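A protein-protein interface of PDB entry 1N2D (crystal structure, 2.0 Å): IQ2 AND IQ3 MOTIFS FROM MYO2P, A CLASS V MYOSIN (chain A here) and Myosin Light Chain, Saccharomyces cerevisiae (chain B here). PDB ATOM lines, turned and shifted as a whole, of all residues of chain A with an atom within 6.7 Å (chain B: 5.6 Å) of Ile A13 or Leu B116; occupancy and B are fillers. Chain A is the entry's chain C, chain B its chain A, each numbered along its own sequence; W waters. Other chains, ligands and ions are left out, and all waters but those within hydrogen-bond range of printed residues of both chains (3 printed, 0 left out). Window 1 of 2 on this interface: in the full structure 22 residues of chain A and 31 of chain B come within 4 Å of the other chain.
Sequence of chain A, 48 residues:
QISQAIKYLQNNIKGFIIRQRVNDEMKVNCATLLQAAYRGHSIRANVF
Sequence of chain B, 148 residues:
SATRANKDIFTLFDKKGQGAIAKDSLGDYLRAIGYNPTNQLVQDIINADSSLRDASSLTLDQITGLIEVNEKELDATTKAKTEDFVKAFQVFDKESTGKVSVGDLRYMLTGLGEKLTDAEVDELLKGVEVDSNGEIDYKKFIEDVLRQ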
ATOM      1  N   ILE A   6      25.932  -3.763  10.120  1.00  0.00           N
ATOM      2  CA  ILE A   6      25.347  -4.307  11.336  1.00  0.00           C
ATOM      3  C   ILE A   6      26.331  -4.210  12.502  1.00  0.00           C
ATOM      4  O   ILE A   6      25.964  -3.755  13.594  1.00  0.00           O
ATOM      5  CB  ILE A   6      24.914  -5.778  11.135  1.00  0.00           C
ATOM      6  CG1 ILE A   6      23.738  -5.829  10.151  1.00  0.00           C
ATOM      7  CG2 ILE A   6      24.514  -6.397  12.474  1.00  0.00           C
ATOM      8  CD1 ILE A   6      23.296  -7.235   9.763  1.00  0.00           C
ATOM      9  N   TYR A   8      28.877  -2.193  12.834  1.00  0.00           N
ATOM     10  CA  TYR A   8      29.059  -0.791  13.186  1.00  0.00           C
ATOM     11  C   TYR A   8      27.883  -0.321  14.031  1.00  0.00           C
ATOM     12  O   TYR A   8      28.062   0.363  15.039  1.00  0.00           O
ATOM     13  CB  TYR A   8      29.175   0.074  11.927  1.00  0.00           C
ATOM     14  CG  TYR A   8      30.579   0.165  11.380  1.00  0.00           C
ATOM     15  CD1 TYR A   8      30.865  -0.210  10.068  1.00  0.00           C
ATOM     16  CD2 TYR A   8      31.626   0.626  12.177  1.00  0.00           C
ATOM     17  CE1 TYR A   8      32.162  -0.133   9.562  1.00  0.00           C
ATOM     18  CE2 TYR A   8      32.924   0.709  11.681  1.00  0.00           C
ATOM     19  CZ  TYR A   8      33.185   0.325  10.376  1.00  0.00           C
ATOM     20  OH  TYR A   8      34.472   0.388   9.891  1.00  0.00           O
ATOM     21  N   LEU A   9      26.677  -0.690  13.617  1.00  0.00           N
ATOM     22  CA  LEU A   9      25.494  -0.306  14.367  1.00  0.00           C
ATOM     23  C   LEU A   9      25.564  -0.884  15.779  1.00  0.00           C
ATOM     24  O   LEU A   9      25.291  -0.186  16.754  1.00  0.00           O
ATOM     25  CB  LEU A   9      24.234  -0.818  13.672  1.00  0.00           C
ATOM     26  CG  LEU A   9      22.913  -0.548  14.402  1.00  0.00           C
ATOM     27  CD1 LEU A   9      22.655   0.947  14.482  1.00  0.00           C
ATOM     28  CD2 LEU A   9      21.782  -1.236  13.658  1.00  0.00           C
ATOM     29  N   GLN A  10      25.946  -2.154  15.888  1.00  0.00           N
ATOM     30  CA  GLN A  10      26.041  -2.794  17.192  1.00  0.00           C
ATOM     31  C   GLN A  10      27.058  -2.095  18.091  1.00  0.00           C
ATOM     32  O   GLN A  10      26.836  -1.993  19.303  1.00  0.00           O
ATOM     33  CB  GLN A  10      26.378  -4.279  17.042  1.00  0.00           C
ATOM     34  CG  GLN A  10      25.253  -5.093  16.409  1.00  0.00           C
ATOM     35  CD  GLN A  10      25.736  -6.430  15.883  1.00  0.00           C
ATOM     36  OE1 GLN A  10      26.795  -6.512  15.270  1.00  0.00           O
ATOM     37  NE2 GLN A  10      24.957  -7.482  16.108  1.00  0.00           N
ATOM     38  N   ASN A  11      28.156  -1.601  17.509  1.00  0.00           N
ATOM     39  CA  ASN A  11      29.174  -0.891  18.297  1.00  0.00           C
ATOM     40  C   ASN A  11      28.587   0.413  18.821  1.00  0.00           C
ATOM     41  O   ASN A  11      28.841   0.823  19.956  1.00  0.00           O
ATOM     42  CB  ASN A  11      30.403  -0.517  17.461  1.00  0.00           C
ATOM     43  CG  ASN A  11      31.091  -1.706  16.839  1.00  0.00           C
ATOM     44  OD1 ASN A  11      31.205  -2.772  17.445  1.00  0.00           O
ATOM     45  ND2 ASN A  11      31.584  -1.518  15.616  1.00  0.00           N
ATOM     46  N   ASN A  12      27.833   1.095  17.970  1.00  0.00           N
ATOM     47  CA  ASN A  12      27.227   2.355  18.374  1.00  0.00           C
ATOM     48  C   ASN A  12      26.124   2.107  19.393  1.00  0.00           C
ATOM     49  O   ASN A  12      25.901   2.920  20.291  1.00  0.00           O
ATOM     50  CB  ASN A  12      26.702   3.095  17.139  1.00  0.00           C
ATOM     51  CG  ASN A  12      27.803   3.866  16.435  1.00  0.00           C
ATOM     52  OD1 ASN A  12      28.156   4.979  16.845  1.00  0.00           O
ATOM     53  ND2 ASN A  12      28.381   3.267  15.399  1.00  0.00           N
ATOM     54  N   ILE A  13      25.447   0.972  19.265  1.00  0.00           N
ATOM     55  CA  ILE A  13      24.392   0.625  20.205  1.00  0.00           C
ATOM     56  C   ILE A  13      24.992   0.354  21.590  1.00  0.00           C
ATOM     57  O   ILE A  13      24.432   0.766  22.604  1.00  0.00           O
ATOM     58  CB  ILE A  13      23.595  -0.588  19.696  1.00  0.00           C
ATOM     59  CG1 ILE A  13      22.602  -0.113  18.629  1.00  0.00           C
ATOM     60  CG2 ILE A  13      22.870  -1.271  20.853  1.00  0.00           C
ATOM     61  CD1 ILE A  13      21.869  -1.225  17.908  1.00  0.00           C
ATOM     62  N   LYS A  14      26.139  -0.319  21.634  1.00  0.00           N
ATOM     63  CA  LYS A  14      26.796  -0.572  22.913  1.00  0.00           C
ATOM     64  C   LYS A  14      27.187   0.755  23.573  1.00  0.00           C
ATOM     65  O   LYS A  14      27.052   0.914  24.782  1.00  0.00           O
ATOM     66  CB  LYS A  14      28.034  -1.445  22.712  1.00  0.00           C
ATOM     67  CG  LYS A  14      27.695  -2.902  22.428  1.00  0.00           C
ATOM     68  CD  LYS A  14      28.901  -3.653  21.882  1.00  0.00           C
ATOM     69  CE  LYS A  14      29.489  -4.597  22.903  1.00  0.00           C
ATOM     70  NZ  LYS A  14      28.537  -5.688  23.255  1.00  0.00           N
ATOM     71  N   GLY A  15      27.675   1.705  22.777  1.00  0.00           N
ATOM     72  CA  GLY A  15      28.042   3.000  23.327  1.00  0.00           C
ATOM     73  C   GLY A  15      26.795   3.688  23.863  1.00  0.00           C
ATOM     74  O   GLY A  15      26.806   4.269  24.948  1.00  0.00           O
ATOM     75  N   PHE A  16      25.711   3.615  23.096  1.00  0.00           N
ATOM     76  CA  PHE A  16      24.441   4.216  23.494  1.00  0.00           C
ATOM     77  C   PHE A  16      23.917   3.642  24.815  1.00  0.00           C
ATOM     78  O   PHE A  16      23.467   4.382  25.694  1.00  0.00           O
ATOM     79  CB  PHE A  16      23.397   3.993  22.397  1.00  0.00           C
ATOM     80  CG  PHE A  16      22.027   4.527  22.738  1.00  0.00           C
ATOM     81  CD1 PHE A  16      21.720   5.869  22.543  1.00  0.00           C
ATOM     82  CD2 PHE A  16      21.054   3.687  23.273  1.00  0.00           C
ATOM     83  CE1 PHE A  16      20.456   6.374  22.878  1.00  0.00           C
ATOM     84  CE2 PHE A  16      19.789   4.179  23.611  1.00  0.00           C
ATOM     85  CZ  PHE A  16      19.491   5.527  23.411  1.00  0.00           C
ATOM     86  N   ILE A  17      23.983   2.322  24.951  1.00  0.00           N
ATOM     87  CA  ILE A  17      23.502   1.643  26.150  1.00  0.00           C
ATOM     88  C   ILE A  17      24.265   2.053  27.397  1.00  0.00           C
ATOM     89  O   ILE A  17      23.664   2.342  28.430  1.00  0.00           O
ATOM     90  CB  ILE A  17      23.599   0.110  25.993  1.00  0.00           C
ATOM     91  CG1 ILE A  17      22.592  -0.363  24.945  1.00  0.00           C
ATOM     92  CG2 ILE A  17      23.384  -0.567  27.335  1.00  0.00           C
ATOM     93  CD1 ILE A  17      22.704  -1.841  24.609  1.00  0.00           C
ATOM     94  N   ILE A  18      25.591   2.079  27.306  1.00  0.00           N
ATOM     95  CA  ILE A  18      26.395   2.454  28.454  1.00  0.00           C
ATOM     96  C   ILE A  18      26.110   3.881  28.880  1.00  0.00           C
ATOM     97  O   ILE A  18      25.922   4.154  30.066  1.00  0.00           O
ATOM     98  CB  ILE A  18      27.904   2.307  28.170  1.00  0.00           C
ATOM     99  CG1 ILE A  18      28.239   0.841  27.881  1.00  0.00           C
ATOM    100  CG2 ILE A  18      28.708   2.810  29.366  1.00  0.00           C
ATOM    101  CD1 ILE A  18      27.858  -0.135  29.011  1.00  0.00           C
ATOM    102  N   ARG A  19      26.071   4.787  27.911  1.00  0.00           N
ATOM    103  CA  ARG A  19      25.812   6.185  28.215  1.00  0.00           C
ATOM    104  C   ARG A  19      24.426   6.376  28.839  1.00  0.00           C
ATOM    105  O   ARG A  19      24.246   7.207  29.740  1.00  0.00           O
ATOM    106  CB  ARG A  19      25.983   7.027  26.947  1.00  0.00           C
ATOM    107  CG  ARG A  19      27.445   7.032  26.445  1.00  0.00           C
ATOM    108  CD  ARG A  19      27.673   8.020  25.305  1.00  0.00           C
ATOM    109  NE  ARG A  19      27.175   7.555  24.007  1.00  0.00           N
ATOM    110  CZ  ARG A  19      27.867   6.792  23.161  1.00  0.00           C
ATOM    111  NH1 ARG A  19      29.100   6.393  23.464  1.00  0.00           N
ATOM    112  NH2 ARG A  19      27.337   6.445  21.993  1.00  0.00           N
ATOM    113  N   LEU B 109      20.046  -7.621  15.673  1.00  0.00           N
ATOM    114  CA  LEU B 109      21.018  -7.297  16.705  1.00  0.00           C
ATOM    115  C   LEU B 109      21.571  -8.497  17.459  1.00  0.00           C
ATOM    116  O   LEU B 109      22.750  -8.509  17.834  1.00  0.00           O
ATOM    117  CB  LEU B 109      20.410  -6.297  17.700  1.00  0.00           C
ATOM    118  CG  LEU B 109      19.985  -4.950  17.103  1.00  0.00           C
ATOM    119  CD1 LEU B 109      19.365  -4.079  18.191  1.00  0.00           C
ATOM    120  CD2 LEU B 109      21.193  -4.253  16.480  1.00  0.00           C
ATOM    121  N   THR B 110      20.737  -9.512  17.668  1.00  0.00           N
ATOM    122  CA  THR B 110      21.173 -10.682  18.418  1.00  0.00           C
ATOM    123  C   THR B 110      21.574 -11.895  17.587  1.00  0.00           C
ATOM    124  O   THR B 110      22.269 -12.781  18.087  1.00  0.00           O
ATOM    125  CB  THR B 110      20.090 -11.132  19.424  1.00  0.00           C
ATOM    126  OG1 THR B 110      18.954 -11.651  18.717  1.00  0.00           O
ATOM    127  CG2 THR B 110      19.651  -9.956  20.277  1.00  0.00           C
ATOM    128  N   GLY B 111      21.145 -11.940  16.330  1.00  0.00           N
ATOM    129  CA  GLY B 111      21.476 -13.087  15.505  1.00  0.00           C
ATOM    130  C   GLY B 111      22.511 -12.847  14.427  1.00  0.00           C
ATOM    131  O   GLY B 111      23.054 -13.801  13.868  1.00  0.00           O
ATOM    132  N   LEU B 112      22.790 -11.581  14.139  1.00  0.00           N
ATOM    133  CA  LEU B 112      23.756 -11.222  13.105  1.00  0.00           C
ATOM    134  C   LEU B 112      24.908 -10.388  13.657  1.00  0.00           C
ATOM    135  O   LEU B 112      24.873  -9.963  14.810  1.00  0.00           O
ATOM    136  CB  LEU B 112      23.052 -10.434  11.994  1.00  0.00           C
ATOM    137  CG  LEU B 112      21.797 -11.074  11.388  1.00  0.00           C
ATOM    138  CD1 LEU B 112      21.179 -10.119  10.382  1.00  0.00           C
ATOM    139  CD2 LEU B 112      22.159 -12.395  10.723  1.00  0.00           C
ATOM    140  N   GLU B 114      28.142  -8.831  15.308  1.00  0.00           N
ATOM    141  CA  GLU B 114      28.746  -9.096  16.618  1.00  0.00           C
ATOM    142  C   GLU B 114      27.577  -9.192  17.588  1.00  0.00           C
ATOM    143  O   GLU B 114      27.283  -8.247  18.316  1.00  0.00           O
ATOM    144  CB  GLU B 114      29.653  -7.938  17.044  1.00  0.00           C
ATOM    145  CG  GLU B 114      30.796  -7.632  16.101  1.00  0.00           C
ATOM    146  CD  GLU B 114      31.513  -6.342  16.469  1.00  0.00           C
ATOM    147  OE1 GLU B 114      30.847  -5.287  16.524  1.00  0.00           O
ATOM    148  OE2 GLU B 114      32.739  -6.382  16.703  1.00  0.00           O
ATOM    149  N   LYS B 115      26.920 -10.344  17.580  1.00  0.00           N
ATOM    150  CA  LYS B 115      25.739 -10.612  18.393  1.00  0.00           C
ATOM    151  C   LYS B 115      25.654  -9.963  19.767  1.00  0.00           C
ATOM    152  O   LYS B 115      26.529 -10.155  20.613  1.00  0.00           O
ATOM    153  CB  LYS B 115      25.572 -12.121  18.554  1.00  0.00           C
ATOM    154  CG  LYS B 115      25.641 -12.882  17.243  1.00  0.00           C
ATOM    155  CD  LYS B 115      25.649 -14.378  17.495  1.00  0.00           C
ATOM    156  CE  LYS B 115      25.824 -15.152  16.207  1.00  0.00           C
ATOM    157  NZ  LYS B 115      25.932 -16.611  16.475  1.00  0.00           N
ATOM    158  N   LEU B 116      24.597  -9.184  19.976  1.00  0.00           N
ATOM    159  CA  LEU B 116      24.363  -8.556  21.276  1.00  0.00           C
ATOM    160  C   LEU B 116      23.428  -9.512  22.010  1.00  0.00           C
ATOM    161  O   LEU B 116      22.800 -10.359  21.386  1.00  0.00           O
ATOM    162  CB  LEU B 116      23.683  -7.196  21.113  1.00  0.00           C
ATOM    163  CG  LEU B 116      24.456  -6.155  20.304  1.00  0.00           C
ATOM    164  CD1 LEU B 116      23.607  -4.900  20.140  1.00  0.00           C
ATOM    165  CD2 LEU B 116      25.786  -5.841  21.001  1.00  0.00           C
ATOM    166  N   THR B 117      23.333  -9.385  23.327  1.00  0.00           N
ATOM    167  CA  THR B 117      22.459 -10.254  24.098  1.00  0.00           C
ATOM    168  C   THR B 117      21.054  -9.683  24.125  1.00  0.00           C
ATOM    169  O   THR B 117      20.842  -8.518  23.793  1.00  0.00           O
ATOM    170  CB  THR B 117      22.916 -10.345  25.557  1.00  0.00           C
ATOM    171  OG1 THR B 117      22.888  -9.026  26.126  1.00  0.00           O
ATOM    172  CG2 THR B 117      24.331 -10.930  25.652  1.00  0.00           C
ATOM    173  N   ASP B 118      20.097 -10.497  24.552  1.00  0.00           N
ATOM    174  CA  ASP B 118      18.727 -10.021  24.657  1.00  0.00           C
ATOM    175  C   ASP B 118      18.653  -8.939  25.729  1.00  0.00           C
ATOM    176  O   ASP B 118      17.875  -7.994  25.608  1.00  0.00           O
ATOM    177  CB  ASP B 118      17.776 -11.174  24.996  1.00  0.00           C
ATOM    178  CG  ASP B 118      17.476 -12.049  23.793  1.00  0.00           C
ATOM    179  OD1 ASP B 118      17.288 -11.492  22.693  1.00  0.00           O
ATOM    180  OD2 ASP B 118      17.415 -13.288  23.944  1.00  0.00           O
ATOM    181  N   GLU B 120      20.926  -6.748  26.409  1.00  0.00           N
ATOM    182  CA  GLU B 120      21.418  -5.506  25.818  1.00  0.00           C
ATOM    183  C   GLU B 120      20.323  -4.867  24.969  1.00  0.00           C
ATOM    184  O   GLU B 120      20.122  -3.649  25.003  1.00  0.00           O
ATOM    185  CB  GLU B 120      22.659  -5.774  24.951  1.00  0.00           C
ATOM    186  CG  GLU B 120      23.934  -6.023  25.756  1.00  0.00           C
ATOM    187  CD  GLU B 120      25.129  -6.363  24.873  1.00  0.00           C
ATOM    188  OE1 GLU B 120      25.082  -7.404  24.181  1.00  0.00           O
ATOM    189  OE2 GLU B 120      26.111  -5.587  24.870  1.00  0.00           O
ATOM    190  N   VAL B 121      19.614  -5.692  24.205  1.00  0.00           N
ATOM    191  CA  VAL B 121      18.546  -5.185  23.360  1.00  0.00           C
ATOM    192  C   VAL B 121      17.423  -4.630  24.229  1.00  0.00           C
ATOM    193  O   VAL B 121      16.862  -3.573  23.935  1.00  0.00           O
ATOM    194  CB  VAL B 121      18.013  -6.283  22.415  1.00  0.00           C
ATOM    195  CG1 VAL B 121      16.715  -5.824  21.742  1.00  0.00           C
ATOM    196  CG2 VAL B 121      19.060  -6.580  21.349  1.00  0.00           C
ATOM    197  N   LEU B 124      18.462  -1.371  25.557  1.00  0.00           N
ATOM    198  CA  LEU B 124      18.385  -0.454  24.423  1.00  0.00           C
ATOM    199  C   LEU B 124      16.945   0.013  24.189  1.00  0.00           C
ATOM    200  O   LEU B 124      16.680   1.210  24.016  1.00  0.00           O
ATOM    201  CB  LEU B 124      18.883  -1.147  23.148  1.00  0.00           C
ATOM    202  CG  LEU B 124      18.501  -0.488  21.814  1.00  0.00           C
ATOM    203  CD1 LEU B 124      19.241   0.836  21.651  1.00  0.00           C
ATOM    204  CD2 LEU B 124      18.842  -1.431  20.653  1.00  0.00           C
ATOM    205  N   PHE B 141      15.296   5.952  15.037  1.00  0.00           N
ATOM    206  CA  PHE B 141      16.046   5.055  15.906  1.00  0.00           C
ATOM    207  C   PHE B 141      17.552   5.298  15.736  1.00  0.00           C
ATOM    208  O   PHE B 141      18.272   5.523  16.711  1.00  0.00           O
ATOM    209  CB  PHE B 141      15.701   3.606  15.553  1.00  0.00           C
ATOM    210  CG  PHE B 141      16.586   2.589  16.211  1.00  0.00           C
ATOM    211  CD1 PHE B 141      16.415   2.257  17.548  1.00  0.00           C
ATOM    212  CD2 PHE B 141      17.608   1.973  15.492  1.00  0.00           C
ATOM    213  CE1 PHE B 141      17.252   1.323  18.165  1.00  0.00           C
ATOM    214  CE2 PHE B 141      18.449   1.040  16.099  1.00  0.00           C
ATOM    215  CZ  PHE B 141      18.270   0.716  17.436  1.00  0.00           C
ATOM    216  N   VAL B 145      20.309   6.757  18.468  1.00  0.00           N
ATOM    217  CA  VAL B 145      21.485   5.968  18.808  1.00  0.00           C
ATOM    218  C   VAL B 145      22.764   6.781  18.615  1.00  0.00           C
ATOM    219  O   VAL B 145      23.642   6.789  19.478  1.00  0.00           O
ATOM    220  CB  VAL B 145      21.562   4.684  17.942  1.00  0.00           C
ATOM    221  CG1 VAL B 145      22.915   3.991  18.129  1.00  0.00           C
ATOM    222  CG2 VAL B 145      20.434   3.740  18.330  1.00  0.00           C
HETATM  223  O   HOH W   1      26.576   6.276  18.831  1.00  0.00           O
HETATM  224  O   HOH W   2      30.450  -3.776  19.515  1.00  0.00           O
HETATM  225  O   HOH W   3      24.975   8.077  21.289  1.00  0.00           O
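The backbone carbonyl oxygen of Leu B109 sits at hydrogen-bond distance from the side-chain amide nitrogen of Gln A10 (3.0 Å). The backbone carbonyl oxygen of Leu B112 sits at hydrogen-bond distance from the side-chain amide nitrogen of Gln A10 (2.8 Å). The side-chain amide oxygen of Gln A10 sits at hydrogen-bond distance from the backbone NH of Glu B114, 2.7 Å away. OD1 of Asn A11 sits close to OE1 of Glu B114 (2.7 Å). The side-chain amino group (NZ) of Lys A14 lies within salt-bridge range of the side-chain carboxylate (OE2) of Glu B120 (2.9 Å).
The backbone carbonyl oxygen (O) of Leu B109 is in hydrogen-bond range of the backbone NH (N) of Leu B116 (2.9 Å). The backbone NH (N) of Thr B117 is in hydrogen-bond range of the side-chain carboxylate (OE1) of Glu B120 (2.8 Å). The side-chain amide oxygen (OE1) of Gln A10 sits close to the backbone carbonyl oxygen (O) of Ile A6, 3.3 Å away. O of Tyr A8 sits at hydrogen-bond distance from ND2 of Asn A12 (2.9 Å).
Among the printed residues, merely in contact across the chains: Ile A17 with Glu B120 (3.2 Å), Ile A13 with Leu B109 (3.4 Å), Lys A14 with Leu B116 (3.6 Å), Ile A6 with Leu B112 (3.6 Å), Phe A16 with Val B145 (3.7 Å), Phe A16 with Leu B124 (3.7 Å), Gln A10 with Lys B115 (3.8 Å), Ile A13 with Leu B116 (3.8 Å) and Asn A12 with Val B145 (3.8 Å).
Ile A13 touches just these residues of chain B: Leu B109 and Leu B116. Leu B116 touches just these residues of chain A: Ile A13 and Lys A14. Printed residues of chain B within 4 Å of Ile A17: Glu B120 (3.2 Å). Of the printed residues of chain B, Gln A10 touches Leu B109, Leu B112, Glu B114 and Lys B115. Of the printed residues of chain A, Glu B120 touches Lys A14 (2.9 Å) and Ile A17 (3.2 Å). Printed residues of chain A within 4 Å of Leu B124: Phe A16. Gly A15 touches none of the printed residues of chain B. The nearest printed residue of chain A that does not touch Leu B124 is Ile A13 (4.04 Å).
Of the 13 printed residues of chain A, 8 touch a printed residue of chain B. Among the printed residues, 14 pairs touch across the chains.
Water W2 lies within hydrogen-bond range of the side-chain amide oxygen of Asn A11 (2.4 Å) and the side-chain carboxylate of Glu B114 (3.4 Å). Water W3 bridges the backbone carbonyl oxygen of Val B145 (2.6 Å) and the guanidinium group of Arg A19 (3.0 Å). Water W1 lies within hydrogen-bond range of OD1 of Asn A12, O of Val B145 and NH2 of Arg A19.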
